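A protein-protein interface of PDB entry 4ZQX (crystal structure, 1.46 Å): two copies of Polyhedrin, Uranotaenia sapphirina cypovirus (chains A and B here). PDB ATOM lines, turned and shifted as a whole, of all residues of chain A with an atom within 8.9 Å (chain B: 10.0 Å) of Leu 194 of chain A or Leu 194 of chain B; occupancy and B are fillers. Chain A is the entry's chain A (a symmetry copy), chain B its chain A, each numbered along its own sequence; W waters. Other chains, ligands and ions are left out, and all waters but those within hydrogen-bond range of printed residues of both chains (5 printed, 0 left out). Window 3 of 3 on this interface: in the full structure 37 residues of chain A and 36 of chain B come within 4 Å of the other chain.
Leu 194 of chain A touches just one residue of chain B: Leu 194 (3.8 Å).
Of chain A, only Leu 194 comes within 4 Å of Leu 194 of chain B.
No residue of chain B comes within 4 Å of Gly 191 of chain A.
Leu 193 of chain A touches none of the printed residues of chain B.
No residue of chain B comes within 4 Å of Gly 195 of chain A.
Val 197 of chain A touches none of the printed residues of chain B.
Of chain A, only Tyr 189 comes within 4 Å of Gly 195 of chain B.
Printed residues of chain B within 4 Å of Tyr 189 of chain A: Gly 195 and Ile 198.
Printed residues of chain B within 4 Å of Val 50 of chain A: Glu 199 (3.6 Å).
Of the printed residues of chain A, Glu 199 of chain B touches Val 50 and Arg 139.
The nearest residue of chain B that does not touch Leu 194 of chain A is Ile 198 of chain B (4.2 Å).
The nearest printed residue of chain A that does not touch Phe 49 of chain B is Val 50 of chain A (11.2 Å).
Water W1 lies within hydrogen-bond range of OE2 of Glu 199 of chain B (2.7 Å), OH of Tyr 189 of chain A (2.8 Å) and O of Phe 49 of chain A (3.1 Å).
Water W3 lies within hydrogen-bond range of O of Pro 192 of chain B (2.8 Å), N of Gly 195 of chain B (3.0 Å) and ND2 of Asn 187 of chain A (3.3 Å).
Water W4 bridges the side-chain carboxylate (OE1) of Glu 199 of chain B (2.8 Å) and the guanidinium group (NH1) of Arg 139 of chain A (2.9 Å).
Water W2 lies within hydrogen-bond range of ND2 of Asn 196 of chain B, OD2 of Asp 24 of chain B and NE of Arg 139 of chain A.
Water W5 bridges the backbone carbonyl oxygen of Gly 191 of chain B and the side-chain amide nitrogen of Asn 187 of chain A.
O of Asn 196 of chain B sits at hydrogen-bond distance from NH1 of Arg 139 of chain A, 2.9 Å away.
The side-chain carboxylate (OD1) of Asp 24 of chain B lies within salt-bridge range of the guanidinium group (NH2) of Arg 139 of chain A.
Tyr 189 of chain A touches Gly 195 of chain B, but with the chains exchanged Gly 195 of chain A does not touch Tyr 189 of chain B (11.4 Å).
Tyr 189 of chain A touches Ile 198 of chain B, but with the chains exchanged Ile 198 of chain A does not touch Tyr 189 of chain B (8.0 Å).
Leu 194 of chain A touches its own counterpart, Leu 194 of chain B.
Leu 201 of chain A touches Ile 198 of chain B, but with the chains exchanged Ile 198 of chain A does not touch Leu 201 of chain B (7.7 Å).
17 positions are printed for both chains.
Of the 10 pairs that touch across the chains among the printed residues, 1 has its exchanged pair printed and touching as well.
The side-chain amide nitrogen of Asn 196 of chain B is in hydrogen-bond range of the side-chain hydroxyl of Tyr 23 of chain B (2.7 Å).
The side-chain amide oxygen of Asn 187 of chain A sits at hydrogen-bond distance from the backbone NH of Tyr 189 of chain A (2.8 Å).
Hydrophobic or aromatic side chains of chain B within 4 Å of the printed part of chain A: Phe 49, Leu 194 and Ile 198.
Of the 19 printed residues of chain A, 5 touch a printed residue of chain B.
Hydrophobic or aromatic side chains of chain A that line the printed part of chain B: Val 50, Tyr 189, Leu 194 and Leu 201.
Among the printed residues, merely in contact across the chains: Leu 201 of chain A with Ile 198 of chain B (3.5 Å), Val 50 of chain A with Glu 199 of chain B (3.6 Å), Arg 139 of chain A with Glu 199 of chain B (3.7 Å), Arg 139 of chain A with Gly 200 of chain B (3.7 Å), Arg 139 of chain A with Phe 49 of chain B (3.8 Å), Leu 194 of chain A with Leu 194 of chain B (3.8 Å), Tyr 189 of chain A with Gly 195 of chain B (3.8 Å) and Tyr 189 of chain A with Ile 198 of chain B (3.8 Å).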
ATOM      1  N   TYR A  23      -7.268  13.254  15.687  1.00  0.00           N
ATOM      2  CA  TYR A  23      -6.780  12.758  16.958  1.00  0.00           C
ATOM      3  C   TYR A  23      -7.400  11.388  17.219  1.00  0.00           C
ATOM      4  O   TYR A  23      -8.598  11.211  17.039  1.00  0.00           O
ATOM      5  CB  TYR A  23      -7.124  13.737  18.086  1.00  0.00           C
ATOM      6  CG  TYR A  23      -6.524  13.337  19.416  1.00  0.00           C
ATOM      7  CD1 TYR A  23      -5.194  13.597  19.707  1.00  0.00           C
ATOM      8  CD2 TYR A  23      -7.291  12.707  20.384  1.00  0.00           C
ATOM      9  CE1 TYR A  23      -4.635  13.225  20.930  1.00  0.00           C
ATOM     10  CE2 TYR A  23      -6.742  12.315  21.604  1.00  0.00           C
ATOM     11  CZ  TYR A  23      -5.415  12.578  21.869  1.00  0.00           C
ATOM     12  OH  TYR A  23      -4.861  12.211  23.069  1.00  0.00           O
ATOM     13  N   PHE A  49      -0.248   7.389  17.686  1.00  0.00           N
ATOM     14  CA  PHE A  49       0.819   8.255  18.206  1.00  0.00           C
ATOM     15  C   PHE A  49       2.230   7.770  17.863  1.00  0.00           C
ATOM     16  O   PHE A  49       3.066   8.540  17.388  1.00  0.00           O
ATOM     17  CB  PHE A  49       0.634   8.389  19.718  1.00  0.00           C
ATOM     18  CG  PHE A  49      -0.748   8.830  20.099  1.00  0.00           C
ATOM     19  CD1 PHE A  49      -1.176  10.104  19.784  1.00  0.00           C
ATOM     20  CD2 PHE A  49      -1.631   7.964  20.733  1.00  0.00           C
ATOM     21  CE1 PHE A  49      -2.454  10.524  20.111  1.00  0.00           C
ATOM     22  CE2 PHE A  49      -2.906   8.383  21.069  1.00  0.00           C
ATOM     23  CZ  PHE A  49      -3.315   9.661  20.754  1.00  0.00           C
ATOM     24  N   VAL A  50       2.496   6.498  18.107  1.00  0.00           N
ATOM     25  CA  VAL A  50       3.748   5.871  17.687  1.00  0.00           C
ATOM     26  C   VAL A  50       3.485   4.427  17.326  1.00  0.00           C
ATOM     27  O   VAL A  50       3.069   3.647  18.185  1.00  0.00           O
ATOM     28  CB  VAL A  50       4.831   5.869  18.809  1.00  0.00           C
ATOM     29  CG1 VAL A  50       6.153   5.470  18.207  1.00  0.00           C
ATOM     30  CG2 VAL A  50       4.936   7.203  19.490  1.00  0.00           C
ATOM     31  N   ARG A 139      17.816   3.438  16.748  1.00  0.00           N
ATOM     32  CA  ARG A 139      17.697   4.631  15.915  1.00  0.00           C
ATOM     33  C   ARG A 139      19.023   5.126  15.354  1.00  0.00           C
ATOM     34  O   ARG A 139      19.386   6.277  15.541  1.00  0.00           O
ATOM     35  CB  ARG A 139      16.978   5.739  16.699  1.00  0.00           C
ATOM     36  CG  ARG A 139      15.545   5.372  16.984  1.00  0.00           C
ATOM     37  CD  ARG A 139      14.753   6.437  17.713  1.00  0.00           C
ATOM     38  NE  ARG A 139      15.193   6.676  19.085  1.00  0.00           N
ATOM     39  CZ  ARG A 139      14.425   7.232  20.021  1.00  0.00           C
ATOM     40  NH1 ARG A 139      13.185   7.609  19.725  1.00  0.00           N
ATOM     41  NH2 ARG A 139      14.895   7.410  21.253  1.00  0.00           N
ATOM     42  N   ASN A 187       2.541  20.245  20.634  1.00  0.00           N
ATOM     43  CA  ASN A 187       3.164  19.065  21.242  1.00  0.00           C
ATOM     44  C   ASN A 187       2.107  18.303  22.026  1.00  0.00           C
ATOM     45  O   ASN A 187       1.656  18.761  23.074  1.00  0.00           O
ATOM     46  CB  ASN A 187       4.333  19.471  22.141  1.00  0.00           C
ATOM     47  CG  ASN A 187       5.022  18.277  22.794  1.00  0.00           C
ATOM     48  OD1 ASN A 187       4.605  17.131  22.610  1.00  0.00           O
ATOM     49  ND2 ASN A 187       6.105  18.541  23.538  1.00  0.00           N
ATOM     50  N   LEU A 188       1.698  17.151  21.502  1.00  0.00           N
ATOM     51  CA  LEU A 188       0.677  16.344  22.158  1.00  0.00           C
ATOM     52  C   LEU A 188       1.135  15.705  23.478  1.00  0.00           C
ATOM     53  O   LEU A 188       0.297  15.254  24.273  1.00  0.00           O
ATOM     54  CB  LEU A 188       0.163  15.254  21.211  1.00  0.00           C
ATOM     55  CG  LEU A 188      -0.571  15.731  19.951  1.00  0.00           C
ATOM     56  CD1 LEU A 188      -1.082  14.528  19.166  1.00  0.00           C
ATOM     57  CD2 LEU A 188      -1.730  16.700  20.286  1.00  0.00           C
ATOM     58  N   TYR A 189       2.445  15.671  23.713  1.00  0.00           N
ATOM     59  CA  TYR A 189       2.999  15.148  24.964  1.00  0.00           C
ATOM     60  C   TYR A 189       3.109  16.226  26.045  1.00  0.00           C
ATOM     61  O   TYR A 189       3.525  15.934  27.161  1.00  0.00           O
ATOM     62  CB  TYR A 189       4.393  14.537  24.749  1.00  0.00           C
ATOM     63  CG  TYR A 189       4.418  13.342  23.828  1.00  0.00           C
ATOM     64  CD1 TYR A 189       4.052  12.080  24.282  1.00  0.00           C
ATOM     65  CD2 TYR A 189       4.810  13.473  22.510  1.00  0.00           C
ATOM     66  CE1 TYR A 189       4.090  10.990  23.447  1.00  0.00           C
ATOM     67  CE2 TYR A 189       4.854  12.382  21.659  1.00  0.00           C
ATOM     68  CZ  TYR A 189       4.485  11.143  22.135  1.00  0.00           C
ATOM     69  OH  TYR A 189       4.525  10.050  21.298  1.00  0.00           O
ATOM     70  N   ALA A 190       2.755  17.461  25.713  1.00  0.00           N
ATOM     71  CA  ALA A 190       2.854  18.570  26.658  1.00  0.00           C
ATOM     72  C   ALA A 190       1.541  18.803  27.371  1.00  0.00           C
ATOM     73  O   ALA A 190       0.474  18.721  26.769  1.00  0.00           O
ATOM     74  CB  ALA A 190       3.277  19.832  25.945  1.00  0.00           C
ATOM     75  N   GLY A 191       1.627  19.099  28.664  1.00  0.00           N
ATOM     76  CA  GLY A 191       0.453  19.442  29.446  1.00  0.00           C
ATOM     77  C   GLY A 191      -0.396  18.230  29.818  1.00  0.00           C
ATOM     78  O   GLY A 191       0.057  17.086  29.751  1.00  0.00           O
ATOM     79  N   PRO A 192      -1.653  18.474  30.207  1.00  0.00           N
ATOM     80  CA  PRO A 192      -2.531  17.407  30.697  1.00  0.00           C
ATOM     81  C   PRO A 192      -2.861  16.327  29.677  1.00  0.00           C
ATOM     82  O   PRO A 192      -3.210  15.246  30.083  1.00  0.00           O
ATOM     83  CB  PRO A 192      -3.810  18.155  31.086  1.00  0.00           C
ATOM     84  CG  PRO A 192      -3.394  19.527  31.321  1.00  0.00           C
ATOM     85  CD  PRO A 192      -2.254  19.804  30.399  1.00  0.00           C
ATOM     86  N   LEU A 193      -2.761  16.613  28.388  1.00  0.00           N
ATOM     87  CA  LEU A 193      -3.058  15.592  27.371  1.00  0.00           C
ATOM     88  C   LEU A 193      -2.135  14.356  27.454  1.00  0.00           C
ATOM     89  O   LEU A 193      -2.482  13.278  26.964  1.00  0.00           O
ATOM     90  CB  LEU A 193      -2.992  16.194  25.969  1.00  0.00           C
ATOM     91  CG  LEU A 193      -3.674  15.379  24.865  1.00  0.00           C
ATOM     92  CD1 LEU A 193      -5.175  15.259  25.092  1.00  0.00           C
ATOM     93  CD2 LEU A 193      -3.399  16.019  23.527  1.00  0.00           C
ATOM     94  N   LEU A 194      -0.963  14.509  28.064  1.00  0.00           N
ATOM     95  CA  LEU A 194       0.032  13.438  28.064  1.00  0.00           C
ATOM     96  C   LEU A 194      -0.523  12.072  28.516  1.00  0.00           C
ATOM     97  O   LEU A 194      -0.303  11.069  27.867  1.00  0.00           O
ATOM     98  CB  LEU A 194       1.235  13.843  28.928  1.00  0.00           C
ATOM     99  CG  LEU A 194       2.291  12.767  29.212  1.00  0.00           C
ATOM    100  CD1 LEU A 194       2.997  12.337  27.923  1.00  0.00           C
ATOM    101  CD2 LEU A 194       3.289  13.290  30.227  1.00  0.00           C
ATOM    102  N   GLY A 195      -1.243  12.042  29.627  1.00  0.00           N
ATOM    103  CA  GLY A 195      -1.801  10.786  30.124  1.00  0.00           C
ATOM    104  C   GLY A 195      -2.701  10.108  29.107  1.00  0.00           C
ATOM    105  O   GLY A 195      -2.731   8.871  28.980  1.00  0.00           O
ATOM    106  N   ASN A 196      -3.458  10.915  28.374  1.00  0.00           N
ATOM    107  CA  ASN A 196      -4.366  10.361  27.368  1.00  0.00           C
ATOM    108  C   ASN A 196      -3.604   9.736  26.192  1.00  0.00           C
ATOM    109  O   ASN A 196      -4.001   8.694  25.660  1.00  0.00           O
ATOM    110  CB  ASN A 196      -5.366  11.426  26.904  1.00  0.00           C
ATOM    111  CG  ASN A 196      -6.529  10.830  26.127  1.00  0.00           C
ATOM    112  OD1 ASN A 196      -7.460  10.252  26.699  1.00  0.00           O
ATOM    113  ND2 ASN A 196      -6.475  10.966  24.824  1.00  0.00           N
ATOM    114  N   VAL A 197      -2.504  10.360  25.803  1.00  0.00           N
ATOM    115  CA  VAL A 197      -1.623   9.786  24.797  1.00  0.00           C
ATOM    116  C   VAL A 197      -0.997   8.485  25.313  1.00  0.00           C
ATOM    117  O   VAL A 197      -0.976   7.484  24.611  1.00  0.00           O
ATOM    118  CB  VAL A 197      -0.521  10.789  24.383  1.00  0.00           C
ATOM    119  CG1 VAL A 197       0.497  10.123  23.454  1.00  0.00           C
ATOM    120  CG2 VAL A 197      -1.140  12.029  23.735  1.00  0.00           C
ATOM    121  N   ILE A 198      -0.495   8.492  26.547  1.00  0.00           N
ATOM    122  CA  ILE A 198       0.170   7.305  27.081  1.00  0.00           C
ATOM    123  C   ILE A 198      -0.806   6.133  27.126  1.00  0.00           C
ATOM    124  O   ILE A 198      -0.440   5.001  26.819  1.00  0.00           O
ATOM    125  CB  ILE A 198       0.801   7.580  28.465  1.00  0.00           C
ATOM    126  CG1 ILE A 198       2.030   8.483  28.294  1.00  0.00           C
ATOM    127  CG2 ILE A 198       1.202   6.273  29.146  1.00  0.00           C
ATOM    128  CD1 ILE A 198       2.678   8.914  29.594  1.00  0.00           C
ATOM    129  N   GLU A 199      -2.056   6.416  27.472  1.00  0.00           N
ATOM    130  CA  GLU A 199      -3.077   5.378  27.544  1.00  0.00           C
ATOM    131  C   GLU A 199      -3.339   4.738  26.187  1.00  0.00           C
ATOM    132  O   GLU A 199      -3.772   3.584  26.119  1.00  0.00           O
ATOM    133  CB  GLU A 199      -4.372   5.959  28.110  1.00  0.00           C
ATOM    134  CG  GLU A 199      -4.303   6.141  29.615  1.00  0.00           C
ATOM    135  CD  GLU A 199      -5.317   7.119  30.173  1.00  0.00           C
ATOM    136  OE1 GLU A 199      -6.191   7.594  29.434  1.00  0.00           O
ATOM    137  OE2 GLU A 199      -5.224   7.423  31.379  1.00  0.00           O
ATOM    138  N   GLY A 200      -3.084   5.479  25.111  1.00  0.00           N
ATOM    139  CA  GLY A 200      -3.383   4.993  23.772  1.00  0.00           C
ATOM    140  C   GLY A 200      -2.265   4.222  23.080  1.00  0.00           C
ATOM    141  O   GLY A 200      -2.489   3.571  22.064  1.00  0.00           O
ATOM    142  N   LEU A 201      -1.059   4.289  23.632  1.00  0.00           N
ATOM    143  CA  LEU A 201       0.082   3.571  23.081  1.00  0.00           C
ATOM    144  C   LEU A 201      -0.118   2.063  23.185  1.00  0.00           C
ATOM    145  O   LEU A 201      -0.566   1.567  24.213  1.00  0.00           O
ATOM    146  CB  LEU A 201       1.341   3.956  23.850  1.00  0.00           C
ATOM    147  CG  LEU A 201       1.792   5.415  23.749  1.00  0.00           C
ATOM    148  CD1 LEU A 201       3.024   5.651  24.602  1.00  0.00           C
ATOM    149  CD2 LEU A 201       2.077   5.799  22.305  1.00  0.00           C
ATOM    150  N   TYR B  23      23.382   8.260  24.777  1.00  0.00           N
ATOM    151  CA  TYR B  23      21.956   8.375  24.547  1.00  0.00           C
ATOM    152  C   TYR B  23      21.568   7.440  23.406  1.00  0.00           C
ATOM    153  O   TYR B  23      22.239   7.408  22.382  1.00  0.00           O
ATOM    154  CB  TYR B  23      21.579   9.825  24.218  1.00  0.00           C
ATOM    155  CG  TYR B  23      20.085  10.031  24.099  1.00  0.00           C
ATOM    156  CD1 TYR B  23      19.290  10.167  25.226  1.00  0.00           C
ATOM    157  CD2 TYR B  23      19.472  10.100  22.857  1.00  0.00           C
ATOM    158  CE1 TYR B  23      17.912  10.352  25.120  1.00  0.00           C
ATOM    159  CE2 TYR B  23      18.093  10.269  22.736  1.00  0.00           C
ATOM    160  CZ  TYR B  23      17.321  10.395  23.872  1.00  0.00           C
ATOM    161  OH  TYR B  23      15.964  10.574  23.772  1.00  0.00           O
ATOM    162  N   ASP B  24      20.491   6.678  23.613  1.00  0.00           N
ATOM    163  CA  ASP B  24      19.989   5.663  22.677  1.00  0.00           C
ATOM    164  C   ASP B  24      20.834   4.377  22.617  1.00  0.00           C
ATOM    165  O   ASP B  24      20.557   3.495  21.799  1.00  0.00           O
ATOM    166  CB  ASP B  24      19.757   6.231  21.260  1.00  0.00           C
ATOM    167  CG  ASP B  24      18.302   6.648  21.007  1.00  0.00           C
ATOM    168  OD1 ASP B  24      17.425   6.508  21.903  1.00  0.00           O
ATOM    169  OD2 ASP B  24      18.054   7.123  19.881  1.00  0.00           O
ATOM    170  N   PHE B  49      16.242   3.020  27.818  1.00  0.00           N
ATOM    171  CA  PHE B  49      15.611   3.831  28.868  1.00  0.00           C
ATOM    172  C   PHE B  49      15.014   3.005  30.010  1.00  0.00           C
ATOM    173  O   PHE B  49      15.252   3.286  31.186  1.00  0.00           O
ATOM    174  CB  PHE B  49      14.550   4.719  28.216  1.00  0.00           C
ATOM    175  CG  PHE B  49      15.087   5.521  27.068  1.00  0.00           C
ATOM    176  CD1 PHE B  49      16.002   6.528  27.299  1.00  0.00           C
ATOM    177  CD2 PHE B  49      14.712   5.244  25.759  1.00  0.00           C
ATOM    178  CE1 PHE B  49      16.523   7.268  26.251  1.00  0.00           C
ATOM    179  CE2 PHE B  49      15.224   5.987  24.709  1.00  0.00           C
ATOM    180  CZ  PHE B  49      16.131   6.994  24.958  1.00  0.00           C
ATOM    181  N   MET B 182      20.454   8.010  35.649  1.00  0.00           N
ATOM    182  CA  MET B 182      20.358   9.455  35.391  1.00  0.00           C
ATOM    183  C   MET B 182      20.998  10.243  36.535  1.00  0.00           C
ATOM    184  O   MET B 182      20.678  11.419  36.758  1.00  0.00           O
ATOM    185  CB  MET B 182      18.895   9.872  35.178  1.00  0.00           C
ATOM    186  CG  MET B 182      18.249   9.163  34.014  1.00  0.00           C
ATOM    187  SD  MET B 182      16.609   9.823  33.627  1.00  0.00           S
ATOM    188  CE  MET B 182      16.076   8.519  32.527  1.00  0.00           C
ATOM    189  N   ASN B 187      17.101  14.968  34.004  1.00  0.00           N
ATOM    190  CA  ASN B 187      15.891  14.150  33.868  1.00  0.00           C
ATOM    191  C   ASN B 187      15.520  14.067  32.396  1.00  0.00           C
ATOM    192  O   ASN B 187      15.074  15.049  31.807  1.00  0.00           O
ATOM    193  CB  ASN B 187      14.746  14.737  34.694  1.00  0.00           C
ATOM    194  CG  ASN B 187      13.461  13.918  34.594  1.00  0.00           C
ATOM    195  OD1 ASN B 187      13.405  12.921  33.870  1.00  0.00           O
ATOM    196  ND2 ASN B 187      12.430  14.322  35.349  1.00  0.00           N
ATOM    197  N   LEU B 188      15.728  12.895  31.800  1.00  0.00           N
ATOM    198  CA  LEU B 188      15.424  12.704  30.387  1.00  0.00           C
ATOM    199  C   LEU B 188      13.923  12.726  30.060  1.00  0.00           C
ATOM    200  O   LEU B 188      13.546  12.876  28.888  1.00  0.00           O
ATOM    201  CB  LEU B 188      16.041  11.397  29.877  1.00  0.00           C
ATOM    202  CG  LEU B 188      17.573  11.313  29.887  1.00  0.00           C
ATOM    203  CD1 LEU B 188      18.021   9.989  29.279  1.00  0.00           C
ATOM    204  CD2 LEU B 188      18.224  12.505  29.145  1.00  0.00           C
ATOM    205  N   TYR B 189      13.077  12.587  31.079  1.00  0.00           N
ATOM    206  CA  TYR B 189      11.626  12.658  30.901  1.00  0.00           C
ATOM    207  C   TYR B 189      11.097  14.090  31.014  1.00  0.00           C
ATOM    208  O   TYR B 189       9.902  14.317  30.856  1.00  0.00           O
ATOM    209  CB  TYR B 189      10.891  11.790  31.936  1.00  0.00           C
ATOM    210  CG  TYR B 189      11.183  10.313  31.836  1.00  0.00           C
ATOM    211  CD1 TYR B 189      10.555   9.521  30.883  1.00  0.00           C
ATOM    212  CD2 TYR B 189      12.082   9.712  32.695  1.00  0.00           C
ATOM    213  CE1 TYR B 189      10.811   8.174  30.803  1.00  0.00           C
ATOM    214  CE2 TYR B 189      12.347   8.355  32.626  1.00  0.00           C
ATOM    215  CZ  TYR B 189      11.711   7.593  31.671  1.00  0.00           C
ATOM    216  OH  TYR B 189      11.967   6.241  31.592  1.00  0.00           O
ATOM    217  N   ALA B 190      11.975  15.044  31.300  1.00  0.00           N
ATOM    218  CA  ALA B 190      11.570  16.437  31.464  1.00  0.00           C
ATOM    219  C   ALA B 190      11.736  17.212  30.176  1.00  0.00           C
ATOM    220  O   ALA B 190      12.711  17.030  29.453  1.00  0.00           O
ATOM    221  CB  ALA B 190      12.376  17.093  32.559  1.00  0.00           C
ATOM    222  N   GLY B 191      10.773  18.085  29.895  1.00  0.00           N
ATOM    223  CA  GLY B 191      10.855  18.963  28.743  1.00  0.00           C
ATOM    224  C   GLY B 191      10.547  18.257  27.425  1.00  0.00           C
ATOM    225  O   GLY B 191       9.969  17.169  27.403  1.00  0.00           O
ATOM    226  N   PRO B 192      10.946  18.872  26.306  1.00  0.00           N
ATOM    227  CA  PRO B 192      10.612  18.353  24.977  1.00  0.00           C
ATOM    228  C   PRO B 192      11.199  16.987  24.654  1.00  0.00           C
ATOM    229  O   PRO B 192      10.664  16.323  23.801  1.00  0.00           O
ATOM    230  CB  PRO B 192      11.201  19.403  24.030  1.00  0.00           C
ATOM    231  CG  PRO B 192      11.296  20.618  24.820  1.00  0.00           C
ATOM    232  CD  PRO B 192      11.564  20.206  26.229  1.00  0.00           C
ATOM    233  N   LEU B 193      12.274  16.582  25.313  1.00  0.00           N
ATOM    234  CA  LEU B 193      12.864  15.262  25.039  1.00  0.00           C
ATOM    235  C   LEU B 193      11.903  14.088  25.328  1.00  0.00           C
ATOM    236  O   LEU B 193      12.079  12.986  24.801  1.00  0.00           O
ATOM    237  CB  LEU B 193      14.159  15.077  25.829  1.00  0.00           C
ATOM    238  CG  LEU B 193      15.081  13.957  25.337  1.00  0.00           C
ATOM    239  CD1 LEU B 193      15.599  14.224  23.930  1.00  0.00           C
ATOM    240  CD2 LEU B 193      16.234  13.800  26.296  1.00  0.00           C
ATOM    241  N   LEU B 194      10.895  14.316  26.165  1.00  0.00           N
ATOM    242  CA  LEU B 194      10.022  13.228  26.607  1.00  0.00           C
ATOM    243  C   LEU B 194       9.451  12.379  25.454  1.00  0.00           C
ATOM    244  O   LEU B 194       9.501  11.166  25.495  1.00  0.00           O
ATOM    245  CB  LEU B 194       8.887  13.791  27.475  1.00  0.00           C
ATOM    246  CG  LEU B 194       7.757  12.829  27.865  1.00  0.00           C
ATOM    247  CD1 LEU B 194       8.279  11.708  28.768  1.00  0.00           C
ATOM    248  CD2 LEU B 194       6.645  13.601  28.547  1.00  0.00           C
ATOM    249  N   GLY B 195       8.915  13.022  24.428  1.00  0.00           N
ATOM    250  CA  GLY B 195       8.349  12.289  23.297  1.00  0.00           C
ATOM    251  C   GLY B 195       9.359  11.366  22.639  1.00  0.00           C
ATOM    252  O   GLY B 195       9.035  10.253  22.191  1.00  0.00           O
ATOM    253  N   ASN B 196      10.602  11.827  22.565  1.00  0.00           N
ATOM    254  CA  ASN B 196      11.651  11.017  21.944  1.00  0.00           C
ATOM    255  C   ASN B 196      11.986   9.775  22.780  1.00  0.00           C
ATOM    256  O   ASN B 196      12.233   8.692  22.239  1.00  0.00           O
ATOM    257  CB  ASN B 196      12.892  11.872  21.662  1.00  0.00           C
ATOM    258  CG  ASN B 196      13.871  11.182  20.725  1.00  0.00           C
ATOM    259  OD1 ASN B 196      13.671  11.128  19.507  1.00  0.00           O
ATOM    260  ND2 ASN B 196      14.927  10.649  21.292  1.00  0.00           N
ATOM    261  N   VAL B 197      11.973   9.928  24.095  1.00  0.00           N
ATOM    262  CA  VAL B 197      12.132   8.793  24.990  1.00  0.00           C
ATOM    263  C   VAL B 197      10.951   7.826  24.845  1.00  0.00           C
ATOM    264  O   VAL B 197      11.141   6.623  24.737  1.00  0.00           O
ATOM    265  CB  VAL B 197      12.273   9.256  26.460  1.00  0.00           C
ATOM    266  CG1 VAL B 197      12.271   8.055  27.409  1.00  0.00           C
ATOM    267  CG2 VAL B 197      13.535  10.104  26.635  1.00  0.00           C
ATOM    268  N   ILE B 198       9.727   8.350  24.830  1.00  0.00           N
ATOM    269  CA  ILE B 198       8.552   7.484  24.755  1.00  0.00           C
ATOM    270  C   ILE B 198       8.581   6.673  23.463  1.00  0.00           C
ATOM    271  O   ILE B 198       8.241   5.492  23.457  1.00  0.00           O
ATOM    272  CB  ILE B 198       7.240   8.289  24.899  1.00  0.00           C
ATOM    273  CG1 ILE B 198       7.090   8.764  26.350  1.00  0.00           C
ATOM    274  CG2 ILE B 198       6.037   7.437  24.499  1.00  0.00           C
ATOM    275  CD1 ILE B 198       5.892   9.659  26.597  1.00  0.00           C
ATOM    276  N   GLU B 199       9.024   7.300  22.381  1.00  0.00           N
ATOM    277  CA  GLU B 199       9.102   6.624  21.091  1.00  0.00           C
ATOM    278  C   GLU B 199      10.080   5.457  21.114  1.00  0.00           C
ATOM    279  O   GLU B 199       9.938   4.512  20.332  1.00  0.00           O
ATOM    280  CB  GLU B 199       9.499   7.621  20.003  1.00  0.00           C
ATOM    281  CG  GLU B 199       8.336   8.503  19.588  1.00  0.00           C
ATOM    282  CD  GLU B 199       8.742   9.786  18.893  1.00  0.00           C
ATOM    283  OE1 GLU B 199       9.928   9.981  18.594  1.00  0.00           O
ATOM    284  OE2 GLU B 199       7.846  10.622  18.653  1.00  0.00           O
ATOM    285  N   GLY B 200      11.072   5.519  22.000  1.00  0.00           N
ATOM    286  CA  GLY B 200      12.109   4.498  22.043  1.00  0.00           C
ATOM    287  C   GLY B 200      11.831   3.308  22.954  1.00  0.00           C
ATOM    288  O   GLY B 200      12.517   2.292  22.883  1.00  0.00           O
ATOM    289  N   LEU B 201      10.822   3.427  23.809  1.00  0.00           N
ATOM    290  CA  LEU B 201      10.440   2.348  24.708  1.00  0.00           C
ATOM    291  C   LEU B 201       9.920   1.145  23.928  1.00  0.00           C
ATOM    292  O   LEU B 201       9.150   1.302  22.988  1.00  0.00           O
ATOM    293  CB  LEU B 201       9.346   2.837  25.649  1.00  0.00           C
ATOM    294  CG  LEU B 201       9.722   3.955  26.623  1.00  0.00           C
ATOM    295  CD1 LEU B 201       8.520   4.363  27.455  1.00  0.00           C
ATOM    296  CD2 LEU B 201      10.864   3.526  27.532  1.00  0.00           C
HETATM  297  O   HOH W   1       5.185  10.448  18.656  1.00  0.00           O
HETATM  298  O   HOH W   2      16.831   9.693  19.338  1.00  0.00           O
HETATM  299  O   HOH W   3       7.911  15.775  23.885  1.00  0.00           O
HETATM  300  O   HOH W   4      11.951   8.516  17.260  1.00  0.00           O
HETATM  301  O   HOH W   5       7.056  16.901  26.400  1.00  0.00           O
